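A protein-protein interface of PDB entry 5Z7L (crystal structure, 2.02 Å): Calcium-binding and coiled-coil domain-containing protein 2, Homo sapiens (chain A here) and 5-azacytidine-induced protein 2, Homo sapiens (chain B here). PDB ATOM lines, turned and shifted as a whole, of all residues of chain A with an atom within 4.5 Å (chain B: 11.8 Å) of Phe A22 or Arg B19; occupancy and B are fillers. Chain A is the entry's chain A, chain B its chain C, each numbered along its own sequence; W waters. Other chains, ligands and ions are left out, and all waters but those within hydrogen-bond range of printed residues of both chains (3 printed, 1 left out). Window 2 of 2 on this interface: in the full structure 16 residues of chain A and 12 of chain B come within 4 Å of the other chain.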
ATOM      1  N   GLU A  20      -8.530   5.143 -23.557  1.00  0.00           N
ATOM      2  CA  GLU A  20      -8.915   6.473 -23.119  1.00  0.00           C
ATOM      3  C   GLU A  20      -9.477   7.279 -24.283  1.00  0.00           C
ATOM      4  O   GLU A  20      -9.224   6.988 -25.452  1.00  0.00           O
ATOM      5  CB  GLU A  20      -7.713   7.199 -22.516  1.00  0.00           C
ATOM      6  CG  GLU A  20      -7.106   6.494 -21.306  1.00  0.00           C
ATOM      7  CD  GLU A  20      -8.004   6.554 -20.075  1.00  0.00           C
ATOM      8  OE1 GLU A  20      -8.925   7.404 -20.040  1.00  0.00           O
ATOM      9  OE2 GLU A  20      -7.786   5.749 -19.139  1.00  0.00           O
ATOM     10  N   LYS A  21     -10.247   8.317 -23.947  1.00  0.00           N
ATOM     11  CA  LYS A  21     -10.678   9.251 -24.981  1.00  0.00           C
ATOM     12  C   LYS A  21      -9.535  10.149 -25.416  1.00  0.00           C
ATOM     13  O   LYS A  21      -9.494  10.585 -26.571  1.00  0.00           O
ATOM     14  CB  LYS A  21     -11.844  10.106 -24.486  1.00  0.00           C
ATOM     15  CG  LYS A  21     -13.071   9.317 -24.137  1.00  0.00           C
ATOM     16  CD  LYS A  21     -14.201  10.237 -23.653  1.00  0.00           C
ATOM     17  CE  LYS A  21     -15.449   9.428 -23.339  1.00  0.00           C
ATOM     18  NZ  LYS A  21     -16.447  10.260 -22.603  1.00  0.00           N
ATOM     19  N   PHE A  22      -8.612  10.445 -24.507  1.00  0.00           N
ATOM     20  CA  PHE A  22      -7.523  11.366 -24.783  1.00  0.00           C
ATOM     21  C   PHE A  22      -6.226  10.819 -24.210  1.00  0.00           C
ATOM     22  O   PHE A  22      -6.206  10.317 -23.087  1.00  0.00           O
ATOM     23  CB  PHE A  22      -7.804  12.748 -24.186  1.00  0.00           C
ATOM     24  CG  PHE A  22      -9.069  13.375 -24.673  1.00  0.00           C
ATOM     25  CD1 PHE A  22      -9.136  13.933 -25.932  1.00  0.00           C
ATOM     26  CD2 PHE A  22     -10.188  13.428 -23.863  1.00  0.00           C
ATOM     27  CE1 PHE A  22     -10.309  14.533 -26.378  1.00  0.00           C
ATOM     28  CE2 PHE A  22     -11.360  14.026 -24.311  1.00  0.00           C
ATOM     29  CZ  PHE A  22     -11.415  14.578 -25.565  1.00  0.00           C
ATOM     30  N   TYR A  23      -5.152  10.911 -24.987  1.00  0.00           N
ATOM     31  CA  TYR A  23      -3.805  10.588 -24.526  1.00  0.00           C
ATOM     32  C   TYR A  23      -2.968  11.861 -24.512  1.00  0.00           C
ATOM     33  O   TYR A  23      -2.878  12.562 -25.526  1.00  0.00           O
ATOM     34  CB  TYR A  23      -3.163   9.509 -25.403  1.00  0.00           C
ATOM     35  CG  TYR A  23      -3.853   8.181 -25.213  1.00  0.00           C
ATOM     36  CD1 TYR A  23      -3.622   7.417 -24.073  1.00  0.00           C
ATOM     37  CD2 TYR A  23      -4.788   7.719 -26.134  1.00  0.00           C
ATOM     38  CE1 TYR A  23      -4.271   6.216 -23.876  1.00  0.00           C
ATOM     39  CE2 TYR A  23      -5.446   6.509 -25.940  1.00  0.00           C
ATOM     40  CZ  TYR A  23      -5.182   5.767 -24.812  1.00  0.00           C
ATOM     41  OH  TYR A  23      -5.838   4.579 -24.613  1.00  0.00           O
ATOM     42  N   ILE A  24      -2.389  12.162 -23.353  1.00  0.00           N
ATOM     43  CA  ILE A  24      -1.510  13.312 -23.135  1.00  0.00           C
ATOM     44  C   ILE A  24      -0.406  13.344 -24.187  1.00  0.00           C
ATOM     45  O   ILE A  24       0.405  12.407 -24.257  1.00  0.00           O
ATOM     46  CB  ILE A  24      -0.891  13.268 -21.728  1.00  0.00           C
ATOM     47  CG1 ILE A  24      -1.980  13.314 -20.654  1.00  0.00           C
ATOM     48  CG2 ILE A  24       0.094  14.422 -21.548  1.00  0.00           C
ATOM     49  CD1 ILE A  24      -2.357  14.714 -20.204  1.00  0.00           C
ATOM     50  N   TYR A  95      -8.807  11.885 -34.863  1.00  0.00           N
ATOM     51  CA  TYR A  95      -9.136  10.676 -34.119  1.00  0.00           C
ATOM     52  C   TYR A  95      -8.313   9.509 -34.650  1.00  0.00           C
ATOM     53  O   TYR A  95      -8.206   9.308 -35.868  1.00  0.00           O
ATOM     54  CB  TYR A  95     -10.622  10.339 -34.234  1.00  0.00           C
ATOM     55  CG  TYR A  95     -11.551  11.172 -33.384  1.00  0.00           C
ATOM     56  CD1 TYR A  95     -11.980  12.419 -33.805  1.00  0.00           C
ATOM     57  CD2 TYR A  95     -12.031  10.691 -32.177  1.00  0.00           C
ATOM     58  CE1 TYR A  95     -12.852  13.178 -33.033  1.00  0.00           C
ATOM     59  CE2 TYR A  95     -12.900  11.439 -31.402  1.00  0.00           C
ATOM     60  CZ  TYR A  95     -13.305  12.675 -31.834  1.00  0.00           C
ATOM     61  OH  TYR A  95     -14.168  13.405 -31.055  1.00  0.00           O
ATOM     62  N   PRO A 113     -11.983   4.957 -30.729  1.00  0.00           N
ATOM     63  CA  PRO A 113     -10.992   5.959 -31.106  1.00  0.00           C
ATOM     64  C   PRO A 113     -10.659   6.926 -29.977  1.00  0.00           C
ATOM     65  O   PRO A 113     -11.362   7.025 -28.965  1.00  0.00           O
ATOM     66  CB  PRO A 113     -11.673   6.690 -32.266  1.00  0.00           C
ATOM     67  CG  PRO A 113     -13.117   6.630 -31.913  1.00  0.00           C
ATOM     68  CD  PRO A 113     -13.340   5.335 -31.174  1.00  0.00           C
ATOM     69  N   GLN A 115      -8.010  10.748 -29.195  1.00  0.00           N
ATOM     70  CA  GLN A 115      -7.233  11.856 -29.704  1.00  0.00           C
ATOM     71  C   GLN A 115      -6.065  12.091 -28.760  1.00  0.00           C
ATOM     72  O   GLN A 115      -6.061  11.638 -27.611  1.00  0.00           O
ATOM     73  CB  GLN A 115      -8.067  13.135 -29.825  1.00  0.00           C
ATOM     74  CG  GLN A 115      -9.140  13.078 -30.877  1.00  0.00           C
ATOM     75  CD  GLN A 115     -10.220  14.079 -30.612  1.00  0.00           C
ATOM     76  OE1 GLN A 115     -10.936  13.979 -29.617  1.00  0.00           O
ATOM     77  NE2 GLN A 115     -10.355  15.058 -31.500  1.00  0.00           N
ATOM     78  N   ARG A 117      -4.535  14.889 -26.932  1.00  0.00           N
ATOM     79  CA  ARG A 117      -4.632  16.249 -26.422  1.00  0.00           C
ATOM     80  C   ARG A 117      -4.520  16.278 -24.893  1.00  0.00           C
ATOM     81  O   ARG A 117      -4.718  15.282 -24.196  1.00  0.00           O
ATOM     82  CB  ARG A 117      -5.934  16.909 -26.882  1.00  0.00           C
ATOM     83  CG  ARG A 117      -7.106  16.740 -25.938  1.00  0.00           C
ATOM     84  CD  ARG A 117      -8.336  17.516 -26.425  1.00  0.00           C
ATOM     85  NE  ARG A 117      -8.536  17.388 -27.867  1.00  0.00           N
ATOM     86  CZ  ARG A 117      -9.651  17.732 -28.501  1.00  0.00           C
ATOM     87  NH1 ARG A 117      -9.741  17.583 -29.815  1.00  0.00           N
ATOM     88  NH2 ARG A 117     -10.685  18.207 -27.820  1.00  0.00           N
ATOM     89  OXT ARG A 117      -4.199  17.315 -24.318  1.00  0.00           O
ATOM     90  N   VAL B  10     -16.738   1.402 -38.467  1.00  0.00           N
ATOM     91  CA  VAL B  10     -17.977   1.183 -37.721  1.00  0.00           C
ATOM     92  C   VAL B  10     -17.688   1.207 -36.228  1.00  0.00           C
ATOM     93  O   VAL B  10     -18.376   1.878 -35.449  1.00  0.00           O
ATOM     94  CB  VAL B  10     -18.637  -0.148 -38.145  1.00  0.00           C
ATOM     95  CG1 VAL B  10     -19.728  -0.576 -37.151  1.00  0.00           C
ATOM     96  CG2 VAL B  10     -19.212  -0.050 -39.546  1.00  0.00           C
ATOM     97  N   THR B  11     -16.643   0.492 -35.813  1.00  0.00           N
ATOM     98  CA  THR B  11     -16.215   0.533 -34.419  1.00  0.00           C
ATOM     99  C   THR B  11     -15.961   1.963 -33.953  1.00  0.00           C
ATOM    100  O   THR B  11     -16.419   2.369 -32.879  1.00  0.00           O
ATOM    101  CB  THR B  11     -14.959  -0.321 -34.239  1.00  0.00           C
ATOM    102  OG1 THR B  11     -15.272  -1.683 -34.521  1.00  0.00           O
ATOM    103  CG2 THR B  11     -14.427  -0.219 -32.793  1.00  0.00           C
ATOM    104  N   ALA B  12     -15.213   2.741 -34.734  1.00  0.00           N
ATOM    105  CA  ALA B  12     -14.995   4.142 -34.362  1.00  0.00           C
ATOM    106  C   ALA B  12     -16.309   4.907 -34.298  1.00  0.00           C
ATOM    107  O   ALA B  12     -16.606   5.577 -33.302  1.00  0.00           O
ATOM    108  CB  ALA B  12     -14.042   4.818 -35.344  1.00  0.00           C
ATOM    109  N   TYR B  13     -17.116   4.817 -35.353  1.00  0.00           N
ATOM    110  CA  TYR B  13     -18.349   5.592 -35.387  1.00  0.00           C
ATOM    111  C   TYR B  13     -19.268   5.226 -34.228  1.00  0.00           C
ATOM    112  O   TYR B  13     -19.882   6.108 -33.615  1.00  0.00           O
ATOM    113  CB  TYR B  13     -19.054   5.389 -36.735  1.00  0.00           C
ATOM    114  CG  TYR B  13     -20.569   5.435 -36.660  1.00  0.00           C
ATOM    115  CD1 TYR B  13     -21.253   6.639 -36.546  1.00  0.00           C
ATOM    116  CD2 TYR B  13     -21.312   4.265 -36.689  1.00  0.00           C
ATOM    117  CE1 TYR B  13     -22.672   6.661 -36.471  1.00  0.00           C
ATOM    118  CE2 TYR B  13     -22.697   4.287 -36.610  1.00  0.00           C
ATOM    119  CZ  TYR B  13     -23.366   5.477 -36.503  1.00  0.00           C
ATOM    120  OH  TYR B  13     -24.746   5.457 -36.439  1.00  0.00           O
ATOM    121  N   GLU B  14     -19.390   3.929 -33.918  1.00  0.00           N
ATOM    122  CA  GLU B  14     -20.307   3.518 -32.853  1.00  0.00           C
ATOM    123  C   GLU B  14     -19.901   4.129 -31.524  1.00  0.00           C
ATOM    124  O   GLU B  14     -20.753   4.563 -30.743  1.00  0.00           O
ATOM    125  CB  GLU B  14     -20.365   1.992 -32.732  1.00  0.00           C
ATOM    126  CG  GLU B  14     -20.943   1.267 -33.939  1.00  0.00           C
ATOM    127  CD  GLU B  14     -22.451   1.160 -33.909  1.00  0.00           C
ATOM    128  OE1 GLU B  14     -23.079   1.873 -33.094  1.00  0.00           O
ATOM    129  OE2 GLU B  14     -23.009   0.356 -34.699  1.00  0.00           O
ATOM    130  N   ASP B  15     -18.601   4.209 -31.258  1.00  0.00           N
ATOM    131  CA  ASP B  15     -18.191   4.840 -30.014  1.00  0.00           C
ATOM    132  C   ASP B  15     -18.357   6.355 -30.051  1.00  0.00           C
ATOM    133  O   ASP B  15     -18.694   6.962 -29.033  1.00  0.00           O
ATOM    134  CB  ASP B  15     -16.756   4.475 -29.672  1.00  0.00           C
ATOM    135  CG  ASP B  15     -16.433   4.778 -28.234  1.00  0.00           C
ATOM    136  OD1 ASP B  15     -16.912   4.029 -27.355  1.00  0.00           O
ATOM    137  OD2 ASP B  15     -15.733   5.777 -27.990  1.00  0.00           O
ATOM    138  N   ILE B  16     -18.115   7.004 -31.191  1.00  0.00           N
ATOM    139  CA  ILE B  16     -18.295   8.454 -31.172  1.00  0.00           C
ATOM    140  C   ILE B  16     -19.780   8.788 -31.061  1.00  0.00           C
ATOM    141  O   ILE B  16     -20.162   9.788 -30.438  1.00  0.00           O
ATOM    142  CB  ILE B  16     -17.640   9.106 -32.397  1.00  0.00           C
ATOM    143  CG1 ILE B  16     -16.114   8.984 -32.293  1.00  0.00           C
ATOM    144  CG2 ILE B  16     -17.990  10.588 -32.456  1.00  0.00           C
ATOM    145  CD1 ILE B  16     -15.399   9.151 -33.613  1.00  0.00           C
ATOM    146  N   LYS B  17     -20.629   7.926 -31.618  1.00  0.00           N
ATOM    147  CA  LYS B  17     -22.073   8.036 -31.453  1.00  0.00           C
ATOM    148  C   LYS B  17     -22.465   7.942 -29.981  1.00  0.00           C
ATOM    149  O   LYS B  17     -23.258   8.751 -29.481  1.00  0.00           O
ATOM    150  CB  LYS B  17     -22.735   6.926 -32.264  1.00  0.00           C
ATOM    151  CG  LYS B  17     -24.218   6.997 -32.335  1.00  0.00           C
ATOM    152  CD  LYS B  17     -24.859   5.654 -32.049  1.00  0.00           C
ATOM    153  CE  LYS B  17     -24.647   4.681 -33.173  1.00  0.00           C
ATOM    154  NZ  LYS B  17     -25.658   3.587 -33.122  1.00  0.00           N
ATOM    155  N   LYS B  18     -21.922   6.949 -29.271  1.00  0.00           N
ATOM    156  CA  LYS B  18     -22.230   6.811 -27.854  1.00  0.00           C
ATOM    157  C   LYS B  18     -21.787   8.048 -27.088  1.00  0.00           C
ATOM    158  O   LYS B  18     -22.509   8.543 -26.216  1.00  0.00           O
ATOM    159  CB  LYS B  18     -21.555   5.560 -27.292  1.00  0.00           C
ATOM    160  CG  LYS B  18     -21.810   5.338 -25.817  1.00  0.00           C
ATOM    161  CD  LYS B  18     -21.065   4.123 -25.287  1.00  0.00           C
ATOM    162  CE  LYS B  18     -19.571   4.230 -25.558  1.00  0.00           C
ATOM    163  NZ  LYS B  18     -18.965   5.447 -24.930  1.00  0.00           N
ATOM    164  N   ARG B  19     -20.603   8.569 -27.412  1.00  0.00           N
ATOM    165  CA  ARG B  19     -20.121   9.781 -26.750  1.00  0.00           C
ATOM    166  C   ARG B  19     -21.046  10.967 -27.002  1.00  0.00           C
ATOM    167  O   ARG B  19     -21.273  11.783 -26.103  1.00  0.00           O
ATOM    168  CB  ARG B  19     -18.707  10.097 -27.220  1.00  0.00           C
ATOM    169  CG  ARG B  19     -17.702   9.086 -26.681  1.00  0.00           C
ATOM    170  CD  ARG B  19     -16.310   9.299 -27.300  1.00  0.00           C
ATOM    171  NE  ARG B  19     -15.718  10.569 -26.893  1.00  0.00           N
ATOM    172  CZ  ARG B  19     -14.490  10.962 -27.232  1.00  0.00           C
ATOM    173  NH1 ARG B  19     -13.726  10.178 -27.976  1.00  0.00           N
ATOM    174  NH2 ARG B  19     -14.028  12.140 -26.838  1.00  0.00           N
ATOM    175  N   LEU B  20     -21.560  11.099 -28.227  1.00  0.00           N
ATOM    176  CA  LEU B  20     -22.501  12.180 -28.511  1.00  0.00           C
ATOM    177  C   LEU B  20     -23.772  12.010 -27.682  1.00  0.00           C
ATOM    178  O   LEU B  20     -24.292  12.982 -27.121  1.00  0.00           O
ATOM    179  CB  LEU B  20     -22.819  12.232 -30.011  1.00  0.00           C
ATOM    180  CG  LEU B  20     -23.858  13.281 -30.433  1.00  0.00           C
ATOM    181  CD1 LEU B  20     -23.426  14.665 -29.971  1.00  0.00           C
ATOM    182  CD2 LEU B  20     -24.113  13.271 -31.935  1.00  0.00           C
ATOM    183  N   LYS B  21     -24.243  10.767 -27.540  1.00  0.00           N
ATOM    184  CA  LYS B  21     -25.417  10.483 -26.713  1.00  0.00           C
ATOM    185  C   LYS B  21     -25.177  10.866 -25.261  1.00  0.00           C
ATOM    186  O   LYS B  21     -26.038  11.486 -24.623  1.00  0.00           O
ATOM    187  CB  LYS B  21     -25.775   9.000 -26.806  1.00  0.00           C
ATOM    188  CG  LYS B  21     -27.148   8.656 -26.253  1.00  0.00           C
ATOM    189  CD  LYS B  21     -27.289   7.140 -26.084  1.00  0.00           C
ATOM    190  CE  LYS B  21     -28.743   6.717 -25.917  1.00  0.00           C
ATOM    191  NZ  LYS B  21     -29.403   6.424 -27.223  1.00  0.00           N
ATOM    192  N   ASP B  22     -24.032  10.459 -24.708  1.00  0.00           N
ATOM    193  CA  ASP B  22     -23.681  10.869 -23.353  1.00  0.00           C
ATOM    194  C   ASP B  22     -23.594  12.379 -23.249  1.00  0.00           C
ATOM    195  O   ASP B  22     -23.993  12.963 -22.238  1.00  0.00           O
ATOM    196  CB  ASP B  22     -22.345  10.251 -22.926  1.00  0.00           C
ATOM    197  CG  ASP B  22     -22.429   8.744 -22.719  1.00  0.00           C
ATOM    198  OD1 ASP B  22     -23.549   8.203 -22.555  1.00  0.00           O
ATOM    199  OD2 ASP B  22     -21.356   8.107 -22.716  1.00  0.00           O
ATOM    200  N   SER B  23     -23.055  13.029 -24.283  1.00  0.00           N
ATOM    201  CA  SER B  23     -22.927  14.484 -24.264  1.00  0.00           C
ATOM    202  C   SER B  23     -24.293  15.172 -24.311  1.00  0.00           C
ATOM    203  O   SER B  23     -24.495  16.199 -23.652  1.00  0.00           O
ATOM    204  CB  SER B  23     -22.044  14.931 -25.438  1.00  0.00           C
ATOM    205  OG  SER B  23     -21.755  16.313 -25.369  1.00  0.00           O
ATOM    206  N   GLU B  24     -25.240  14.639 -25.097  1.00  0.00           N
ATOM    207  CA  GLU B  24     -26.580  15.226 -25.097  1.00  0.00           C
ATOM    208  C   GLU B  24     -27.270  15.021 -23.752  1.00  0.00           C
ATOM    209  O   GLU B  24     -28.037  15.880 -23.310  1.00  0.00           O
ATOM    210  CB  GLU B  24     -27.448  14.619 -26.219  1.00  0.00           C
ATOM    211  CG  GLU B  24     -26.872  14.713 -27.636  1.00  0.00           C
ATOM    212  CD  GLU B  24     -27.680  13.910 -28.675  1.00  0.00           C
ATOM    213  OE1 GLU B  24     -28.392  12.939 -28.303  1.00  0.00           O
ATOM    214  OE2 GLU B  24     -27.607  14.254 -29.875  1.00  0.00           O
ATOM    215  N   LYS B  25     -27.040  13.878 -23.098  1.00  0.00           N
ATOM    216  CA  LYS B  25     -27.690  13.669 -21.809  1.00  0.00           C
ATOM    217  C   LYS B  25     -27.123  14.622 -20.766  1.00  0.00           C
ATOM    218  O   LYS B  25     -27.879  15.220 -19.997  1.00  0.00           O
ATOM    219  CB  LYS B  25     -27.574  12.205 -21.374  1.00  0.00           C
ATOM    220  CG  LYS B  25     -28.271  11.266 -22.370  1.00  0.00           C
ATOM    221  CD  LYS B  25     -27.891   9.790 -22.197  1.00  0.00           C
ATOM    222  CE  LYS B  25     -28.844   8.851 -22.956  1.00  0.00           C
ATOM    223  NZ  LYS B  25     -30.126   9.475 -23.417  1.00  0.00           N
ATOM    224  N   GLU B  26     -25.803  14.828 -20.759  1.00  0.00           N
ATOM    225  CA  GLU B  26     -25.249  15.840 -19.868  1.00  0.00           C
ATOM    226  C   GLU B  26     -25.765  17.231 -20.224  1.00  0.00           C
ATOM    227  O   GLU B  26     -26.134  18.007 -19.334  1.00  0.00           O
ATOM    228  CB  GLU B  26     -23.723  15.808 -19.902  1.00  0.00           C
ATOM    229  CG  GLU B  26     -23.088  16.474 -18.680  1.00  0.00           C
ATOM    230  CD  GLU B  26     -21.635  16.853 -18.899  1.00  0.00           C
ATOM    231  OE1 GLU B  26     -21.092  16.547 -19.984  1.00  0.00           O
ATOM    232  OE2 GLU B  26     -21.040  17.459 -17.981  1.00  0.00           O
ATOM    233  N   ASN B  27     -25.815  17.558 -21.518  1.00  0.00           N
ATOM    234  CA  ASN B  27     -26.425  18.816 -21.953  1.00  0.00           C
ATOM    235  C   ASN B  27     -27.812  18.980 -21.351  1.00  0.00           C
ATOM    236  O   ASN B  27     -28.174  20.060 -20.865  1.00  0.00           O
ATOM    237  CB  ASN B  27     -26.495  18.851 -23.484  1.00  0.00           C
ATOM    238  CG  ASN B  27     -26.864  20.225 -24.045  1.00  0.00           C
ATOM    239  OD1 ASN B  27     -28.024  20.470 -24.413  1.00  0.00           O
ATOM    240  ND2 ASN B  27     -25.869  21.109 -24.165  1.00  0.00           N
ATOM    241  N   SER B  28     -28.599  17.907 -21.353  1.00  0.00           N
ATOM    242  CA  SER B  28     -29.971  18.027 -20.884  1.00  0.00           C
ATOM    243  C   SER B  28     -30.008  18.192 -19.363  1.00  0.00           C
ATOM    244  O   SER B  28     -30.813  18.968 -18.843  1.00  0.00           O
ATOM    245  CB  SER B  28     -30.785  16.821 -21.359  1.00  0.00           C
ATOM    246  OG  SER B  28     -31.886  16.592 -20.513  1.00  0.00           O
ATOM    247  N   LEU B  30     -27.512  19.586 -17.549  1.00  0.00           N
ATOM    248  CA  LEU B  30     -27.030  20.932 -17.275  1.00  0.00           C
ATOM    249  C   LEU B  30     -28.148  21.956 -17.433  1.00  0.00           C
ATOM    250  O   LEU B  30     -28.302  22.853 -16.596  1.00  0.00           O
ATOM    251  CB  LEU B  30     -25.854  21.260 -18.188  1.00  0.00           C
ATOM    252  CG  LEU B  30     -24.602  20.419 -17.863  1.00  0.00           C
ATOM    253  CD1 LEU B  30     -23.520  20.647 -18.929  1.00  0.00           C
ATOM    254  CD2 LEU B  30     -24.077  20.690 -16.442  1.00  0.00           C
HETATM  255  O   HOH W   1     -18.832   9.418 -22.871  1.00  0.00           O
HETATM  256  O   HOH W   2     -11.384  11.767 -28.266  1.00  0.00           O
HETATM  257  O   HOH W   3     -14.127   7.559 -28.771  1.00  0.00           O
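O of Lys A21 sits at hydrogen-bond distance from N of Gln A115, at 3.0 Å.
OD1 of Asp B15 lies within salt-bridge range of NZ of Lys B18 (3.5 Å).
Among the printed residues, pairs that only touch across the chains: Lys A21 with Arg B19, Tyr A95 with Arg B19, Pro A113 with Ala B12, Phe A22 with Arg B19, Pro A113 with Ile B16, Pro A113 with Asp B15 and Tyr A95 with Ile B16.
Glu A20 touches none of the printed residues of chain B.
No residue of chain B comes within 4 Å of Ile A24.
Of chain B, only Ala B12 (3.8 Å), Asp B15 (3.8 Å) and Ile B16 (3.8 Å) come within 4 Å of Pro A113.
No residue of chain B comes within 4 Å of Gln A115.
Arg A117 touches none of the printed residues of chain B.
Of the printed residues of chain A, Ala B12 touches Pro A113 (3.8 Å).
Printed residues of chain A within 4 Å of Ile B16: Tyr A95 (3.97 Å) and Pro A113 (3.8 Å).
Of chain A, only Lys A21 (3.6 Å), Phe A22 (3.8 Å) and Tyr A95 (3.7 Å) come within 4 Å of Arg B19.
The nearest residue of chain B that does not touch Phe A22 is Asp B15 (9.2 Å).
The nearest residue of chain A that does not touch Arg B19 is Pro A113 (4.1 Å).
Hydrophobic or aromatic side chains of chain A that line the printed part of chain B: Phe A22, Tyr A95 and Pro A113.
Of the 20 printed residues of chain B, 4 touch a printed residue of chain A.
Hydrophobic or aromatic side chains of chain B within 4 Å of the printed part of chain A: Ala B12 and Ile B16.
Among the printed residues, no Asp or Glu carboxylate lies within 4 Å of a Lys or Arg side-chain nitrogen of the other chain.
Water W3 lies within hydrogen-bond range of OD2 of Asp B15 (2.5 Å), NH1 of Arg B19 (2.8 Å) and O of Pro A113 (2.8 Å).
Water W1 lies within hydrogen-bond range of the side-chain amino group of Lys A21 (2.5 Å) and the side-chain carboxylate of Asp B22 (2.8 Å).
Water W2 lies within hydrogen-bond range of the side-chain amide oxygen of Gln A115 (2.6 Å), the backbone carbonyl oxygen of Lys A21 (2.8 Å) and the guanidinium group of Arg B19 (2.8 Å).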
